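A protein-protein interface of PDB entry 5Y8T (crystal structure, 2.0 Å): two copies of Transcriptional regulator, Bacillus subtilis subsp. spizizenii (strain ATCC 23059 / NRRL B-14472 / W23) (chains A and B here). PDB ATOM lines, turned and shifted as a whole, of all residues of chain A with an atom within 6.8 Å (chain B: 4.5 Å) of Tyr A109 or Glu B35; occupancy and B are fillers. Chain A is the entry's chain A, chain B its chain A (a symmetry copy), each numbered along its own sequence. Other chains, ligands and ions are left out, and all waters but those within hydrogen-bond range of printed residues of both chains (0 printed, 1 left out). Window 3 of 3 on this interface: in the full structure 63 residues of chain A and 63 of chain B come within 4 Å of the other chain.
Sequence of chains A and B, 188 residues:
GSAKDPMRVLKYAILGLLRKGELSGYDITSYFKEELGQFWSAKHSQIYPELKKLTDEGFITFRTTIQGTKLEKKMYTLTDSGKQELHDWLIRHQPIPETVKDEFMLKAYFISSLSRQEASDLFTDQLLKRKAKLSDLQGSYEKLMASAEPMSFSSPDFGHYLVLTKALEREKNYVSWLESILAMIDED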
ATOM      1  N   PHE A 104      -4.096  18.748   6.677  1.00  0.00           N
ATOM      2  CA  PHE A 104      -3.123  17.659   6.453  1.00  0.00           C
ATOM      3  C   PHE A 104      -3.566  16.352   7.146  1.00  0.00           C
ATOM      4  O   PHE A 104      -3.431  15.275   6.602  1.00  0.00           O
ATOM      5  CB  PHE A 104      -1.729  18.054   6.935  1.00  0.00           C
ATOM      6  CG  PHE A 104      -0.733  16.947   6.768  1.00  0.00           C
ATOM      7  CD1 PHE A 104      -0.211  16.677   5.511  1.00  0.00           C
ATOM      8  CD2 PHE A 104      -0.396  16.132   7.825  1.00  0.00           C
ATOM      9  CE1 PHE A 104       0.656  15.629   5.323  1.00  0.00           C
ATOM     10  CE2 PHE A 104       0.485  15.059   7.641  1.00  0.00           C
ATOM     11  CZ  PHE A 104       1.012  14.814   6.384  1.00  0.00           C
ATOM     12  N   MET A 105      -4.100  16.477   8.351  1.00  0.00           N
ATOM     13  CA  MET A 105      -4.496  15.305   9.121  1.00  0.00           C
ATOM     14  C   MET A 105      -5.696  14.603   8.550  1.00  0.00           C
ATOM     15  O   MET A 105      -5.825  13.406   8.713  1.00  0.00           O
ATOM     16  CB  MET A 105      -4.653  15.691  10.594  1.00  0.00           C
ATOM     17  CG  MET A 105      -3.297  15.960  11.272  1.00  0.00           C
ATOM     18  SD  MET A 105      -2.036  14.700  11.129  1.00  0.00           S
ATOM     19  CE  MET A 105      -2.928  13.249  11.737  1.00  0.00           C
ATOM     20  N   LEU A 106      -6.568  15.342   7.854  1.00  0.00           N
ATOM     21  CA  LEU A 106      -7.697  14.770   7.162  1.00  0.00           C
ATOM     22  C   LEU A 106      -7.170  13.919   6.054  1.00  0.00           C
ATOM     23  O   LEU A 106      -7.645  12.825   5.853  1.00  0.00           O
ATOM     24  CB  LEU A 106      -8.648  15.865   6.628  1.00  0.00           C
ATOM     25  CG  LEU A 106      -9.996  15.402   6.133  1.00  0.00           C
ATOM     26  CD1 LEU A 106     -10.776  14.617   7.229  1.00  0.00           C
ATOM     27  CD2 LEU A 106     -10.842  16.590   5.514  1.00  0.00           C
ATOM     28  N   LYS A 107      -6.153  14.404   5.342  1.00  0.00           N
ATOM     29  CA  LYS A 107      -5.503  13.577   4.328  1.00  0.00           C
ATOM     30  C   LYS A 107      -4.918  12.295   4.917  1.00  0.00           C
ATOM     31  O   LYS A 107      -5.089  11.205   4.360  1.00  0.00           O
ATOM     32  CB  LYS A 107      -4.394  14.368   3.611  1.00  0.00           C
ATOM     33  CG  LYS A 107      -4.920  15.576   2.909  1.00  0.00           C
ATOM     34  CD  LYS A 107      -3.821  16.245   2.092  1.00  0.00           C
ATOM     35  CE  LYS A 107      -4.347  17.506   1.399  1.00  0.00           C
ATOM     36  NZ  LYS A 107      -3.259  18.079   0.554  1.00  0.00           N
ATOM     37  N   ALA A 108      -4.223  12.440   6.033  1.00  0.00           N
ATOM     38  CA  ALA A 108      -3.623  11.299   6.707  1.00  0.00           C
ATOM     39  C   ALA A 108      -4.721  10.305   7.081  1.00  0.00           C
ATOM     40  O   ALA A 108      -4.544   9.107   6.929  1.00  0.00           O
ATOM     41  CB  ALA A 108      -2.869  11.754   7.989  1.00  0.00           C
ATOM     42  N   TYR A 109      -5.862  10.798   7.558  1.00  0.00           N
ATOM     43  CA  TYR A 109      -6.991   9.896   7.843  1.00  0.00           C
ATOM     44  C   TYR A 109      -7.412   9.049   6.635  1.00  0.00           C
ATOM     45  O   TYR A 109      -7.822   7.894   6.779  1.00  0.00           O
ATOM     46  CB  TYR A 109      -8.161  10.710   8.325  1.00  0.00           C
ATOM     47  CG  TYR A 109      -9.315   9.884   8.848  1.00  0.00           C
ATOM     48  CD1 TYR A 109      -9.185   9.080   9.970  1.00  0.00           C
ATOM     49  CD2 TYR A 109     -10.534   9.950   8.244  1.00  0.00           C
ATOM     50  CE1 TYR A 109     -10.272   8.320  10.474  1.00  0.00           C
ATOM     51  CE2 TYR A 109     -11.616   9.201   8.720  1.00  0.00           C
ATOM     52  CZ  TYR A 109     -11.475   8.407   9.847  1.00  0.00           C
ATOM     53  OH  TYR A 109     -12.533   7.694  10.292  1.00  0.00           O
ATOM     54  N   PHE A 110      -7.315   9.632   5.449  1.00  0.00           N
ATOM     55  CA  PHE A 110      -7.692   8.976   4.202  1.00  0.00           C
ATOM     56  C   PHE A 110      -6.494   8.352   3.470  1.00  0.00           C
ATOM     57  O   PHE A 110      -6.556   8.136   2.278  1.00  0.00           O
ATOM     58  CB  PHE A 110      -8.412   9.977   3.294  1.00  0.00           C
ATOM     59  CG  PHE A 110      -9.695  10.524   3.891  1.00  0.00           C
ATOM     60  CD1 PHE A 110     -10.631   9.677   4.402  1.00  0.00           C
ATOM     61  CD2 PHE A 110      -9.948  11.876   3.916  1.00  0.00           C
ATOM     62  CE1 PHE A 110     -11.813  10.168   4.975  1.00  0.00           C
ATOM     63  CE2 PHE A 110     -11.117  12.374   4.455  1.00  0.00           C
ATOM     64  CZ  PHE A 110     -12.041  11.513   5.004  1.00  0.00           C
ATOM     65  N   ILE A 111      -5.429   8.029   4.207  1.00  0.00           N
ATOM     66  CA  ILE A 111      -4.174   7.580   3.595  1.00  0.00           C
ATOM     67  C   ILE A 111      -4.342   6.301   2.735  1.00  0.00           C
ATOM     68  O   ILE A 111      -3.559   6.102   1.784  1.00  0.00           O
ATOM     69  CB  ILE A 111      -3.084   7.394   4.671  1.00  0.00           C
ATOM     70  CG1 ILE A 111      -1.685   7.235   4.009  1.00  0.00           C
ATOM     71  CG2 ILE A 111      -3.448   6.293   5.601  1.00  0.00           C
ATOM     72  CD1 ILE A 111      -0.472   7.321   4.972  1.00  0.00           C
ATOM     73  N   SER A 112      -5.365   5.489   3.032  1.00  0.00           N
ATOM     74  CA  SER A 112      -5.663   4.269   2.258  1.00  0.00           C
ATOM     75  C   SER A 112      -5.835   4.550   0.779  1.00  0.00           C
ATOM     76  O   SER A 112      -5.632   3.645  -0.036  1.00  0.00           O
ATOM     77  CB  SER A 112      -6.936   3.543   2.757  1.00  0.00           C
ATOM     78  OG  SER A 112      -8.122   4.316   2.507  1.00  0.00           O
ATOM     79  N   PHE A 123       3.990  13.198   2.994  1.00  0.00           N
ATOM     80  CA  PHE A 123       4.540  13.345   4.321  1.00  0.00           C
ATOM     81  C   PHE A 123       5.891  14.028   4.312  1.00  0.00           C
ATOM     82  O   PHE A 123       6.178  14.778   5.240  1.00  0.00           O
ATOM     83  CB  PHE A 123       4.600  12.035   5.035  1.00  0.00           C
ATOM     84  CG  PHE A 123       3.292  11.682   5.711  1.00  0.00           C
ATOM     85  CD1 PHE A 123       2.164  11.491   4.964  1.00  0.00           C
ATOM     86  CD2 PHE A 123       3.197  11.631   7.061  1.00  0.00           C
ATOM     87  CE1 PHE A 123       0.931  11.167   5.588  1.00  0.00           C
ATOM     88  CE2 PHE A 123       1.982  11.356   7.701  1.00  0.00           C
ATOM     89  CZ  PHE A 123       0.863  11.106   6.944  1.00  0.00           C
ATOM     90  N   ARG B  19     -14.887   6.804   0.159  1.00  0.00           N
ATOM     91  CA  ARG B  19     -13.777   6.269  -0.638  1.00  0.00           C
ATOM     92  C   ARG B  19     -13.781   4.762  -0.605  1.00  0.00           C
ATOM     93  O   ARG B  19     -13.275   4.151  -1.530  1.00  0.00           O
ATOM     94  CB  ARG B  19     -12.419   6.797  -0.168  1.00  0.00           C
ATOM     95  CG  ARG B  19     -11.852   6.100   1.070  1.00  0.00           C
ATOM     96  CD  ARG B  19     -10.805   6.915   1.776  1.00  0.00           C
ATOM     97  NE  ARG B  19     -10.189   6.176   2.871  1.00  0.00           N
ATOM     98  CZ  ARG B  19     -10.730   6.016   4.068  1.00  0.00           C
ATOM     99  NH1 ARG B  19     -11.928   6.534   4.360  1.00  0.00           N
ATOM    100  NH2 ARG B  19     -10.077   5.322   4.983  1.00  0.00           N
ATOM    101  N   TYR B  31     -20.854   8.631  10.819  1.00  0.00           N
ATOM    102  CA  TYR B  31     -19.354   8.680  10.817  1.00  0.00           C
ATOM    103  C   TYR B  31     -18.782   9.940  11.471  1.00  0.00           C
ATOM    104  O   TYR B  31     -17.689   9.909  12.058  1.00  0.00           O
ATOM    105  CB  TYR B  31     -18.731   8.506   9.410  1.00  0.00           C
ATOM    106  CG  TYR B  31     -18.520   7.064   9.014  1.00  0.00           C
ATOM    107  CD1 TYR B  31     -17.692   6.233   9.763  1.00  0.00           C
ATOM    108  CD2 TYR B  31     -19.154   6.526   7.895  1.00  0.00           C
ATOM    109  CE1 TYR B  31     -17.507   4.891   9.419  1.00  0.00           C
ATOM    110  CE2 TYR B  31     -18.969   5.189   7.529  1.00  0.00           C
ATOM    111  CZ  TYR B  31     -18.145   4.375   8.296  1.00  0.00           C
ATOM    112  OH  TYR B  31     -17.967   3.050   7.956  1.00  0.00           O
ATOM    113  N   GLU B  34     -18.539   9.678  15.233  1.00  0.00           N
ATOM    114  CA  GLU B  34     -17.504   8.769  15.753  1.00  0.00           C
ATOM    115  C   GLU B  34     -16.128   9.471  15.732  1.00  0.00           C
ATOM    116  O   GLU B  34     -16.004  10.604  16.203  1.00  0.00           O
ATOM    117  CB  GLU B  34     -17.496   7.432  14.975  1.00  0.00           C
ATOM    118  N   GLU B  35     -15.120   8.792  15.184  1.00  0.00           N
ATOM    119  CA  GLU B  35     -13.715   9.223  15.254  1.00  0.00           C
ATOM    120  C   GLU B  35     -13.396  10.389  14.330  1.00  0.00           C
ATOM    121  O   GLU B  35     -12.517  11.198  14.622  1.00  0.00           O
ATOM    122  CB  GLU B  35     -12.790   8.041  14.911  1.00  0.00           C
ATOM    123  CG  GLU B  35     -12.853   7.643  13.460  1.00  0.00           C
ATOM    124  CD  GLU B  35     -12.811   6.165  13.206  1.00  0.00           C
ATOM    125  OE1 GLU B  35     -13.495   5.414  13.912  1.00  0.00           O
ATOM    126  OE2 GLU B  35     -12.122   5.760  12.242  1.00  0.00           O
ATOM    127  N   LEU B  36     -14.094  10.450  13.201  1.00  0.00           N
ATOM    128  CA  LEU B  36     -13.902  11.544  12.262  1.00  0.00           C
ATOM    129  C   LEU B  36     -14.249  12.868  12.935  1.00  0.00           C
ATOM    130  O   LEU B  36     -13.548  13.845  12.732  1.00  0.00           O
ATOM    131  CB  LEU B  36     -14.732  11.338  10.980  1.00  0.00           C
ATOM    132  CG  LEU B  36     -14.616  12.386   9.862  1.00  0.00           C
ATOM    133  CD1 LEU B  36     -13.171  12.659   9.477  1.00  0.00           C
ATOM    134  CD2 LEU B  36     -15.433  11.960   8.625  1.00  0.00           C
ATOM    135  N   GLY B  37     -15.307  12.888  13.753  1.00  0.00           N
ATOM    136  CA  GLY B  37     -15.766  14.108  14.430  1.00  0.00           C
ATOM    137  C   GLY B  37     -14.951  14.606  15.628  1.00  0.00           C
ATOM    138  O   GLY B  37     -15.277  15.638  16.214  1.00  0.00           O
ATOM    139  N   GLN B  38     -13.916  13.876  16.027  1.00  0.00           N
ATOM    140  CA  GLN B  38     -12.991  14.384  17.026  1.00  0.00           C
ATOM    141  C   GLN B  38     -12.022  15.415  16.432  1.00  0.00           C
ATOM    142  O   GLN B  38     -11.619  16.340  17.102  1.00  0.00           O
ATOM    143  CB  GLN B  38     -12.218  13.234  17.659  1.00  0.00           C
ATOM    144  CG  GLN B  38     -13.064  12.309  18.526  1.00  0.00           C
ATOM    145  CD  GLN B  38     -13.777  13.053  19.612  1.00  0.00           C
ATOM    146  OE1 GLN B  38     -13.153  13.435  20.626  1.00  0.00           O
ATOM    147  NE2 GLN B  38     -15.101  13.258  19.422  1.00  0.00           N
ATOM    148  N   PHE B  39     -11.663  15.278  15.161  1.00  0.00           N
ATOM    149  CA  PHE B  39     -10.651  16.173  14.593  1.00  0.00           C
ATOM    150  C   PHE B  39     -11.189  16.936  13.379  1.00  0.00           C
ATOM    151  O   PHE B  39     -10.528  17.826  12.831  1.00  0.00           O
ATOM    152  CB  PHE B  39      -9.397  15.360  14.259  1.00  0.00           C
ATOM    153  CG  PHE B  39      -9.595  14.368  13.121  1.00  0.00           C
ATOM    154  CD1 PHE B  39     -10.079  13.091  13.373  1.00  0.00           C
ATOM    155  CD2 PHE B  39      -9.307  14.715  11.823  1.00  0.00           C
ATOM    156  CE1 PHE B  39     -10.264  12.188  12.346  1.00  0.00           C
ATOM    157  CE2 PHE B  39      -9.511  13.803  10.791  1.00  0.00           C
ATOM    158  CZ  PHE B  39      -9.997  12.549  11.066  1.00  0.00           C
ATOM    159  N   GLY B 159      -5.001   4.924   8.917  1.00  0.00           N
ATOM    160  CA  GLY B 159      -5.437   6.338   8.931  1.00  0.00           C
ATOM    161  C   GLY B 159      -5.950   6.747  10.300  1.00  0.00           C
ATOM    162  O   GLY B 159      -5.643   7.837  10.831  1.00  0.00           O
ATOM    163  N   HIS B 160      -6.749   5.868  10.904  1.00  0.00           N
ATOM    164  CA  HIS B 160      -7.216   6.112  12.271  1.00  0.00           C
ATOM    165  C   HIS B 160      -6.029   6.217  13.271  1.00  0.00           C
ATOM    166  O   HIS B 160      -5.983   7.098  14.161  1.00  0.00           O
ATOM    167  CB  HIS B 160      -8.176   4.954  12.614  1.00  0.00           C
ATOM    168  CG  HIS B 160      -8.952   5.147  13.875  1.00  0.00           C
ATOM    169  ND1 HIS B 160     -10.062   4.387  14.175  1.00  0.00           N
ATOM    170  CD2 HIS B 160      -8.809   6.030  14.893  1.00  0.00           C
ATOM    171  CE1 HIS B 160     -10.549   4.769  15.343  1.00  0.00           C
ATOM    172  NE2 HIS B 160      -9.829   5.789  15.782  1.00  0.00           N
ATOM    173  N   VAL B 163      -4.419   9.741  12.965  1.00  0.00           N
ATOM    174  CA  VAL B 163      -5.094  10.863  13.611  1.00  0.00           C
ATOM    175  C   VAL B 163      -5.064  10.704  15.135  1.00  0.00           C
ATOM    176  O   VAL B 163      -4.964  11.695  15.882  1.00  0.00           O
ATOM    177  CB  VAL B 163      -6.492  11.078  13.081  1.00  0.00           C
ATOM    178  CG1 VAL B 163      -6.466  11.451  11.625  1.00  0.00           C
ATOM    179  CG2 VAL B 163      -7.397   9.845  13.293  1.00  0.00           C
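Among the printed residues, merely in contact across the chains: Phe A110 with Arg B19, Ala A108 with Gly B159, Tyr A109 with Phe B39, Met A105 with Val B163, Tyr A109 with Gly B159, Tyr A109 with Val B163, Leu A106 with Leu B36, Tyr A109 with Arg B19, Tyr A109 with Leu B36, Leu A106 with Phe B39 and Ile A111 with Gly B159.
Tyr A109 touches six residues of chain B.
Glu B35 touches just one residue of chain A: Tyr A109.
Of the printed residues of chain A, Phe B39 touches Leu A106 (3.9 Å) and Tyr A109 (3.5 Å).
Of the printed residues of chain B, Ala A108 touches Gly B159.
Printed residues of chain B within 4 Å of Ser A112: Arg B19.
Of the printed residues of chain B, Phe A110 touches Arg B19 (3.4 Å).
Gln B38 touches none of the printed residues of chain A.
Phe A123 touches none of the printed residues of chain B.
The nearest printed residue of chain A that does not touch Glu B35 is Leu A106 (8.3 Å).
No position is printed for both chains.
Of the 13 pairs that touch across the chains among the printed residues, none has its exchanged pair printed and touching as well.
ND1 of His B160 sits at hydrogen-bond distance from OE2 of Glu B35 (3.1 Å).
The side-chain carboxylate (OE2) of Glu B35 lies within hydrogen-bond range of the side-chain hydroxyl (OH) of Tyr A109.
The side-chain hydroxyl (OG) of Ser A112 is in hydrogen-bond range of the guanidinium group (NE) of Arg B19 (2.8 Å).
Of the 11 printed residues of chain B, 6 touch a printed residue of chain A.
Printed residues of chain B that touch a printed residue of chain A: Arg B19, Glu B35, Leu B36, Phe B39, Gly B159 and Val B163.
Hydrophobic or aromatic side chains of chain B within 4 Å of the printed part of chain A: Leu B36, Phe B39 and Val B163.
Along chain B the printed residues that touch a printed residue of chain A span positions 19 to 163.
Among the printed residues, no Asp or Glu carboxylate lies within 4 Å of a Lys or Arg side-chain nitrogen of the other chain.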
